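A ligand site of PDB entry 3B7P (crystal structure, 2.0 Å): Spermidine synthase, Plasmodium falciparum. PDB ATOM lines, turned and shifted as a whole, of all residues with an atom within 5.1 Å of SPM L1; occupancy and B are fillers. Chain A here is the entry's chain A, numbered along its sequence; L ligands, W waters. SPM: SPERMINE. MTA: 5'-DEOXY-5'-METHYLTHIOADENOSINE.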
ATOM      1  N   GLU A   8     -21.508   9.652  30.809  1.00  0.00           N
ATOM      2  CA  GLU A   8     -21.766   8.755  29.689  1.00  0.00           C
ATOM      3  C   GLU A   8     -23.239   8.351  29.615  1.00  0.00           C
ATOM      4  O   GLU A   8     -23.667   7.371  30.236  1.00  0.00           O
ATOM      5  CB  GLU A   8     -20.854   7.525  29.790  1.00  0.00           C
ATOM      6  CG  GLU A   8     -20.779   6.686  28.526  1.00  0.00           C
ATOM      7  CD  GLU A   8     -20.089   5.350  28.773  1.00  0.00           C
ATOM      8  OE1 GLU A   8     -20.302   4.759  29.861  1.00  0.00           O
ATOM      9  OE2 GLU A   8     -19.345   4.891  27.876  1.00  0.00           O
ATOM     10  N   TRP A  13     -27.781   2.360  26.451  1.00  0.00           N
ATOM     11  CA  TRP A  13     -28.055   1.976  27.847  1.00  0.00           C
ATOM     12  C   TRP A  13     -28.904   3.046  28.553  1.00  0.00           C
ATOM     13  O   TRP A  13     -28.414   3.780  29.413  1.00  0.00           O
ATOM     14  CB  TRP A  13     -26.759   1.702  28.614  1.00  0.00           C
ATOM     15  CG  TRP A  13     -25.646   2.699  28.340  1.00  0.00           C
ATOM     16  CD1 TRP A  13     -25.363   3.821  29.043  1.00  0.00           C
ATOM     17  CD2 TRP A  13     -24.682   2.629  27.275  1.00  0.00           C
ATOM     18  NE1 TRP A  13     -24.286   4.474  28.481  1.00  0.00           N
ATOM     19  CE2 TRP A  13     -23.843   3.752  27.406  1.00  0.00           C
ATOM     20  CE3 TRP A  13     -24.437   1.716  26.232  1.00  0.00           C
ATOM     21  CZ2 TRP A  13     -22.776   3.997  26.525  1.00  0.00           C
ATOM     22  CZ3 TRP A  13     -23.395   1.963  25.368  1.00  0.00           C
ATOM     23  CH2 TRP A  13     -22.574   3.100  25.518  1.00  0.00           C
ATOM     24  N   VAL A  53     -18.963   8.175  24.223  1.00  0.00           N
ATOM     25  CA  VAL A  53     -18.783   6.836  24.814  1.00  0.00           C
ATOM     26  C   VAL A  53     -17.323   6.620  25.233  1.00  0.00           C
ATOM     27  O   VAL A  53     -16.403   6.816  24.440  1.00  0.00           O
ATOM     28  CB  VAL A  53     -19.203   5.705  23.849  1.00  0.00           C
ATOM     29  CG1 VAL A  53     -18.951   4.326  24.478  1.00  0.00           C
ATOM     30  CG2 VAL A  53     -20.670   5.845  23.435  1.00  0.00           C
ATOM     31  N   ILE A  54     -17.135   6.220  26.488  1.00  0.00           N
ATOM     32  CA  ILE A  54     -15.800   5.920  26.996  1.00  0.00           C
ATOM     33  C   ILE A  54     -15.214   4.735  26.236  1.00  0.00           C
ATOM     34  O   ILE A  54     -15.856   3.676  26.136  1.00  0.00           O
ATOM     35  CB  ILE A  54     -15.825   5.594  28.510  1.00  0.00           C
ATOM     36  CG1 ILE A  54     -16.395   6.785  29.292  1.00  0.00           C
ATOM     37  CG2 ILE A  54     -14.424   5.169  28.989  1.00  0.00           C
ATOM     38  CD1 ILE A  54     -16.648   6.522  30.779  1.00  0.00           C
ATOM     39  N   GLN A  55     -14.002   4.916  25.715  1.00  0.00           N
ATOM     40  CA  GLN A  55     -13.311   3.859  24.967  1.00  0.00           C
ATOM     41  C   GLN A  55     -12.264   3.218  25.850  1.00  0.00           C
ATOM     42  O   GLN A  55     -12.074   2.007  25.844  1.00  0.00           O
ATOM     43  CB  GLN A  55     -12.665   4.447  23.695  1.00  0.00           C
ATOM     44  CG  GLN A  55     -13.647   5.161  22.795  1.00  0.00           C
ATOM     45  CD  GLN A  55     -14.656   4.223  22.146  1.00  0.00           C
ATOM     46  OE1 GLN A  55     -15.876   4.457  22.196  1.00  0.00           O
ATOM     47  NE2 GLN A  55     -14.156   3.176  21.515  1.00  0.00           N
ATOM     48  N   LEU A  56     -11.572   4.020  26.630  1.00  0.00           N
ATOM     49  CA  LEU A  56     -10.637   3.467  27.573  1.00  0.00           C
ATOM     50  C   LEU A  56     -10.303   4.485  28.641  1.00  0.00           C
ATOM     51  O   LEU A  56     -10.575   5.671  28.473  1.00  0.00           O
ATOM     52  CB  LEU A  56      -9.355   2.959  26.869  1.00  0.00           C
ATOM     53  CG  LEU A  56      -8.467   3.944  26.088  1.00  0.00           C
ATOM     54  CD1 LEU A  56      -7.550   4.785  26.982  1.00  0.00           C
ATOM     55  CD2 LEU A  56      -7.617   3.163  25.116  1.00  0.00           C
ATOM     56  N   TYR A  64      -9.363  -5.068  29.570  1.00  0.00           N
ATOM     57  CA  TYR A  64      -9.972  -5.287  28.271  1.00  0.00           C
ATOM     58  C   TYR A  64      -8.975  -5.714  27.188  1.00  0.00           C
ATOM     59  O   TYR A  64      -9.264  -6.605  26.387  1.00  0.00           O
ATOM     60  CB  TYR A  64     -10.666  -4.013  27.838  1.00  0.00           C
ATOM     61  CG  TYR A  64     -11.228  -4.068  26.444  1.00  0.00           C
ATOM     62  CD1 TYR A  64     -12.475  -4.659  26.197  1.00  0.00           C
ATOM     63  CD2 TYR A  64     -10.521  -3.538  25.379  1.00  0.00           C
ATOM     64  CE1 TYR A  64     -12.994  -4.702  24.911  1.00  0.00           C
ATOM     65  CE2 TYR A  64     -11.038  -3.580  24.082  1.00  0.00           C
ATOM     66  CZ  TYR A  64     -12.273  -4.157  23.859  1.00  0.00           C
ATOM     67  OH  TYR A  64     -12.764  -4.192  22.587  1.00  0.00           O
ATOM     68  N   HIS A  65      -7.806  -5.070  27.144  1.00  0.00           N
ATOM     69  CA  HIS A  65      -6.858  -5.355  26.083  1.00  0.00           C
ATOM     70  C   HIS A  65      -6.186  -6.707  26.276  1.00  0.00           C
ATOM     71  O   HIS A  65      -5.999  -7.440  25.297  1.00  0.00           O
ATOM     72  CB  HIS A  65      -5.863  -4.198  25.894  1.00  0.00           C
ATOM     73  CG  HIS A  65      -6.510  -2.929  25.437  1.00  0.00           C
ATOM     74  ND1 HIS A  65      -6.323  -1.722  26.101  1.00  0.00           N
ATOM     75  CD2 HIS A  65      -7.357  -2.673  24.417  1.00  0.00           C
ATOM     76  CE1 HIS A  65      -7.019  -0.782  25.487  1.00  0.00           C
ATOM     77  NE2 HIS A  65      -7.660  -1.331  24.466  1.00  0.00           N
ATOM     78  N   GLY A  87      -9.559  -0.590  16.921  1.00  0.00           N
ATOM     79  CA  GLY A  87      -8.428  -0.594  17.854  1.00  0.00           C
ATOM     80  C   GLY A  87      -7.378   0.496  17.719  1.00  0.00           C
ATOM     81  O   GLY A  87      -6.219   0.278  18.097  1.00  0.00           O
ATOM     82  N   ASP A  89      -6.425   3.031  19.306  1.00  0.00           N
ATOM     83  CA  ASP A  89      -5.617   3.412  20.490  1.00  0.00           C
ATOM     84  C   ASP A  89      -4.311   2.615  20.641  1.00  0.00           C
ATOM     85  O   ASP A  89      -3.349   3.086  21.265  1.00  0.00           O
ATOM     86  CB  ASP A  89      -6.485   3.289  21.749  1.00  0.00           C
ATOM     87  CG  ASP A  89      -7.193   1.954  21.826  1.00  0.00           C
ATOM     88  OD1 ASP A  89      -6.541   0.971  22.199  1.00  0.00           O
ATOM     89  OD2 ASP A  89      -8.379   1.889  21.458  1.00  0.00           O
ATOM     90  N   ASP A 158     -11.715  -4.993  17.647  1.00  0.00           N
ATOM     91  CA  ASP A 158     -11.727  -4.036  18.744  1.00  0.00           C
ATOM     92  C   ASP A 158     -12.443  -2.758  18.308  1.00  0.00           C
ATOM     93  O   ASP A 158     -11.838  -1.697  18.161  1.00  0.00           O
ATOM     94  CB  ASP A 158     -10.297  -3.726  19.221  1.00  0.00           C
ATOM     95  CG  ASP A 158     -10.252  -2.751  20.387  1.00  0.00           C
ATOM     96  OD1 ASP A 158     -11.285  -2.530  21.038  1.00  0.00           O
ATOM     97  OD2 ASP A 158      -9.174  -2.185  20.680  1.00  0.00           O
ATOM     98  N   SER A 159     -13.755  -2.877  18.112  1.00  0.00           N
ATOM     99  CA  SER A 159     -14.574  -1.799  17.590  1.00  0.00           C
ATOM    100  C   SER A 159     -15.143  -0.928  18.687  1.00  0.00           C
ATOM    101  O   SER A 159     -15.226  -1.332  19.854  1.00  0.00           O
ATOM    102  CB  SER A 159     -15.738  -2.386  16.799  1.00  0.00           C
ATOM    103  OG  SER A 159     -16.617  -3.106  17.657  1.00  0.00           O
ATOM    104  N   SER A 160     -15.547   0.282  18.300  1.00  0.00           N
ATOM    105  CA  SER A 160     -16.476   1.072  19.080  1.00  0.00           C
ATOM    106  C   SER A 160     -17.880   0.449  18.952  1.00  0.00           C
ATOM    107  O   SER A 160     -18.058  -0.609  18.328  1.00  0.00           O
ATOM    108  CB  SER A 160     -16.449   2.529  18.615  1.00  0.00           C
ATOM    109  OG  SER A 160     -16.513   2.625  17.197  1.00  0.00           O
ATOM    110  N   ASP A 161     -18.882   1.092  19.552  1.00  0.00           N
ATOM    111  CA  ASP A 161     -20.254   0.562  19.565  1.00  0.00           C
ATOM    112  C   ASP A 161     -21.005   0.738  18.230  1.00  0.00           C
ATOM    113  O   ASP A 161     -20.559   1.506  17.386  1.00  0.00           O
ATOM    114  CB  ASP A 161     -21.012   1.201  20.723  1.00  0.00           C
ATOM    115  CG  ASP A 161     -20.422   0.836  22.056  1.00  0.00           C
ATOM    116  OD1 ASP A 161     -20.312  -0.374  22.352  1.00  0.00           O
ATOM    117  OD2 ASP A 161     -20.064   1.761  22.818  1.00  0.00           O
ATOM    118  N   GLN A 191     -15.510  -7.540  20.282  1.00  0.00           N
ATOM    119  CA  GLN A 191     -16.197  -6.844  21.342  1.00  0.00           C
ATOM    120  C   GLN A 191     -17.675  -7.091  21.176  1.00  0.00           C
ATOM    121  O   GLN A 191     -18.200  -6.930  20.123  1.00  0.00           O
ATOM    122  CB  GLN A 191     -15.887  -5.354  21.241  1.00  0.00           C
ATOM    123  CG  GLN A 191     -16.511  -4.448  22.282  1.00  0.00           C
ATOM    124  CD  GLN A 191     -17.794  -3.817  21.842  1.00  0.00           C
ATOM    125  OE1 GLN A 191     -18.827  -4.160  22.297  1.00  0.00           O
ATOM    126  NE2 GLN A 191     -17.711  -2.893  20.968  1.00  0.00           N
ATOM    127  N   CYS A 192     -18.320  -7.517  22.246  1.00  0.00           N
ATOM    128  CA  CYS A 192     -19.742  -7.780  22.238  1.00  0.00           C
ATOM    129  C   CYS A 192     -20.439  -7.121  23.436  1.00  0.00           C
ATOM    130  O   CYS A 192     -19.806  -6.602  24.302  1.00  0.00           O
ATOM    131  CB  CYS A 192     -19.984  -9.277  22.186  1.00  0.00           C
ATOM    132  SG  CYS A 192     -21.348  -9.790  21.231  1.00  0.00           S
ATOM    133  N   GLU A 193     -21.738  -7.049  23.445  1.00  0.00           N
ATOM    134  CA  GLU A 193     -22.422  -6.118  24.338  1.00  0.00           C
ATOM    135  C   GLU A 193     -22.040  -6.322  25.854  1.00  0.00           C
ATOM    136  O   GLU A 193     -21.079  -6.982  26.168  1.00  0.00           O
ATOM    137  CB  GLU A 193     -23.927  -6.139  24.020  1.00  0.00           C
ATOM    138  CG  GLU A 193     -24.937  -5.738  25.099  1.00  0.00           C
ATOM    139  CD  GLU A 193     -25.181  -4.252  25.226  1.00  0.00           C
ATOM    140  OE1 GLU A 193     -24.281  -3.514  25.626  1.00  0.00           O
ATOM    141  OE2 GLU A 193     -26.283  -3.818  24.990  1.00  0.00           O
ATOM    142  N   SER A 194     -22.767  -5.732  26.771  1.00  0.00           N
ATOM    143  CA  SER A 194     -22.757  -6.223  28.138  1.00  0.00           C
ATOM    144  C   SER A 194     -23.890  -7.163  28.352  1.00  0.00           C
ATOM    145  O   SER A 194     -24.986  -6.892  27.945  1.00  0.00           O
ATOM    146  CB  SER A 194     -22.882  -5.080  29.089  1.00  0.00           C
ATOM    147  OG  SER A 194     -22.767  -5.536  30.392  1.00  0.00           O
ATOM    148  N   TYR A 226     -16.741   0.602  31.431  1.00  0.00           N
ATOM    149  CA  TYR A 226     -17.745   0.292  30.406  1.00  0.00           C
ATOM    150  C   TYR A 226     -19.107   0.133  31.090  1.00  0.00           C
ATOM    151  O   TYR A 226     -19.164  -0.262  32.272  1.00  0.00           O
ATOM    152  CB  TYR A 226     -17.383  -0.965  29.592  1.00  0.00           C
ATOM    153  CG  TYR A 226     -16.196  -0.796  28.651  1.00  0.00           C
ATOM    154  CD1 TYR A 226     -15.846   0.451  28.117  1.00  0.00           C
ATOM    155  CD2 TYR A 226     -15.441  -1.902  28.274  1.00  0.00           C
ATOM    156  CE1 TYR A 226     -14.748   0.590  27.254  1.00  0.00           C
ATOM    157  CE2 TYR A 226     -14.349  -1.775  27.409  1.00  0.00           C
ATOM    158  CZ  TYR A 226     -14.011  -0.532  26.893  1.00  0.00           C
ATOM    159  OH  TYR A 226     -12.921  -0.438  26.046  1.00  0.00           O
ATOM    160  N   PRO A 227     -20.207   0.460  30.384  1.00  0.00           N
ATOM    161  CA  PRO A 227     -21.543   0.395  30.976  1.00  0.00           C
ATOM    162  C   PRO A 227     -21.817  -0.967  31.605  1.00  0.00           C
ATOM    163  O   PRO A 227     -21.559  -1.998  30.992  1.00  0.00           O
ATOM    164  CB  PRO A 227     -22.468   0.618  29.771  1.00  0.00           C
ATOM    165  CG  PRO A 227     -21.662   1.358  28.793  1.00  0.00           C
ATOM    166  CD  PRO A 227     -20.236   0.956  28.994  1.00  0.00           C
ATOM    167  N   ILE A 231     -17.826  -6.161  29.836  1.00  0.00           N
ATOM    168  CA  ILE A 231     -18.031  -6.311  28.393  1.00  0.00           C
ATOM    169  C   ILE A 231     -17.722  -7.749  27.955  1.00  0.00           C
ATOM    170  O   ILE A 231     -16.891  -8.435  28.543  1.00  0.00           O
ATOM    171  CB  ILE A 231     -17.221  -5.235  27.578  1.00  0.00           C
ATOM    172  CG1 ILE A 231     -17.830  -5.043  26.182  1.00  0.00           C
ATOM    173  CG2 ILE A 231     -15.715  -5.534  27.533  1.00  0.00           C
ATOM    174  CD1 ILE A 231     -17.546  -3.701  25.603  1.00  0.00           C
HETATM  175  N1  SPM L   1     -21.532  -2.632  23.678  1.00  0.00           N
HETATM  176  C2  SPM L   1     -22.042  -1.837  24.829  1.00  0.00           C
HETATM  177  C3  SPM L   1     -20.910  -1.316  25.753  1.00  0.00           C
HETATM  178  C4  SPM L   1     -20.582   0.163  25.431  1.00  0.00           C
HETATM  179  N5  SPM L   1     -19.169   0.578  25.588  1.00  0.00           N
HETATM  180  C6  SPM L   1     -18.247  -0.245  24.785  1.00  0.00           C
HETATM  181  C7  SPM L   1     -17.030   0.557  24.312  1.00  0.00           C
HETATM  182  C8  SPM L   1     -16.148  -0.342  23.448  1.00  0.00           C
HETATM  183  C9  SPM L   1     -14.930   0.400  22.890  1.00  0.00           C
HETATM  184  N10 SPM L   1     -13.859  -0.572  22.594  1.00  0.00           N
HETATM  185  C11 SPM L   1     -12.706   0.055  21.940  1.00  0.00           C
HETATM  186  C12 SPM L   1     -11.852   0.853  22.923  1.00  0.00           C
HETATM  187  C13 SPM L   1     -10.743   0.025  23.581  1.00  0.00           C
HETATM  188  N14 SPM L   1      -9.660  -0.270  22.629  1.00  0.00           N
HETATM  189  CS  MTA L   2     -10.893   3.279  20.197  1.00  0.00           C
HETATM  190  S5' MTA L   2     -10.704   1.647  19.569  1.00  0.00           S
HETATM  191  C5' MTA L   2     -12.174   1.394  18.615  1.00  0.00           C
HETATM  192  C4' MTA L   2     -11.971   1.914  17.198  1.00  0.00           C
HETATM  193  O4' MTA L   2     -12.899   1.322  16.267  1.00  0.00           O
HETATM  194  C2' MTA L   2     -13.087   3.539  15.808  1.00  0.00           C
HETATM  195  O2' MTA L   2     -12.681   4.652  14.990  1.00  0.00           O
HETATM  196  C3' MTA L   2     -12.251   3.402  17.067  1.00  0.00           C
HETATM  197  O3' MTA L   2     -11.038   4.125  16.922  1.00  0.00           O
HETATM  198  C1' MTA L   2     -12.857   2.184  15.162  1.00  0.00           C
HETATM  199  N9  MTA L   2     -13.878   1.826  14.142  1.00  0.00           N
HETATM  200  C8  MTA L   2     -15.198   2.037  14.197  1.00  0.00           C
HETATM  201  N7  MTA L   2     -15.811   1.593  13.055  1.00  0.00           N
HETATM  202  C5  MTA L   2     -14.838   1.070  12.256  1.00  0.00           C
HETATM  203  C6  MTA L   2     -14.755   0.434  10.925  1.00  0.00           C
HETATM  204  N6  MTA L   2     -15.877   0.229  10.163  1.00  0.00           N
HETATM  205  N1  MTA L   2     -13.527   0.062  10.494  1.00  0.00           N
HETATM  206  C2  MTA L   2     -12.397   0.260  11.216  1.00  0.00           C
HETATM  207  N3  MTA L   2     -12.401   0.839  12.434  1.00  0.00           N
HETATM  208  C4  MTA L   2     -13.563   1.242  12.987  1.00  0.00           C
HETATM  209  O   HOH W   1     -18.218   2.587  27.123  1.00  0.00           O
HETATM  210  O   HOH W   2     -20.266  -2.518  28.609  1.00  0.00           O
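N14 of SPM L1 sits at hydrogen-bond distance from NE2 of His 65 (2.9 Å).
A nitrogen (N1) of SPM L1 is in hydrogen-bond range of the side-chain amide oxygen (OE1) of Gln 191 (3.4 Å).
N14 of SPM L1 lies within salt-bridge range of OD2 of Asp 158 (2.8 Å).
N1 of SPM L1 lies within salt-bridge range of OE1 of Glu 193.
The side-chain carboxylate (OD2) of Asp 89 lies within salt-bridge range of a nitrogen (N14) of SPM L1 (2.8 Å).
The backbone NH (N) of Gly 87 lies close to a sulfur (S5') of MTA L2, at 3.7 Å.
OD1 of Asp 161 lies within salt-bridge range of N1 of SPM L1.
The backbone NH (N) of Ser 160 is in hydrogen-bond range of an oxygen (O4') of MTA L2 (3.5 Å).
O of Ser 159 lies within hydrogen-bond range of N10 of SPM L1 (3.2 Å).
A nitrogen (N14) of SPM L1 lies close to a sulfur (S5') of MTA L2 (3.8 Å).
The backbone carbonyl oxygen (O) of Val 53 lies close to the side-chain amide oxygen (OE1) of Gln 55.
OD1 of Asp 89 is in hydrogen-bond range of NE2 of His 65 (3.4 Å).
OD1 of Asp 158 is in hydrogen-bond range of OH of Tyr 64, at 2.7 Å.
The backbone carbonyl oxygen (O) of Ser 159 lies within hydrogen-bond range of the side-chain amide nitrogen (NE2) of Gln 191 (3.1 Å).
O of Asp 158 is in hydrogen-bond range of N of Gly 87 (2.8 Å).
The side-chain hydroxyl of Tyr 226 sits at hydrogen-bond distance from the backbone carbonyl oxygen of Gln 55.
The side-chain carboxylate (OE2) of Glu 8 sits at hydrogen-bond distance from the backbone NH (N) of Ile 54 (2.9 Å).
The backbone carbonyl oxygen (O) of Glu 8 is in hydrogen-bond range of the indole nitrogen (NE1) of Trp 13.
Residues that only touch SPM L1: Gln 55 (3.1 Å), Tyr 226 (3.3 Å), Trp 13 (3.3 Å), Pro 227 (3.6 Å), Ile 231 (3.6 Å), Tyr 64 (3.7 Å), Ile 54 (3.8 Å) and Val 53 (3.9 Å).
Hydrophobic or aromatic side chains that line SPM L1: Trp 13, Val 53, Tyr 64, His 65, Tyr 226, Pro 227 and Ile 231.
Of the 21 residues printed, 15 come within 4 Å of SPM L1.
The nearest printed residue that does not touch SPM L1 is Ser 160 (4.2 Å).
Water W1 lies within hydrogen-bond range of OE2 of Glu 8, N5 of SPM L1 and O of Ile 54.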
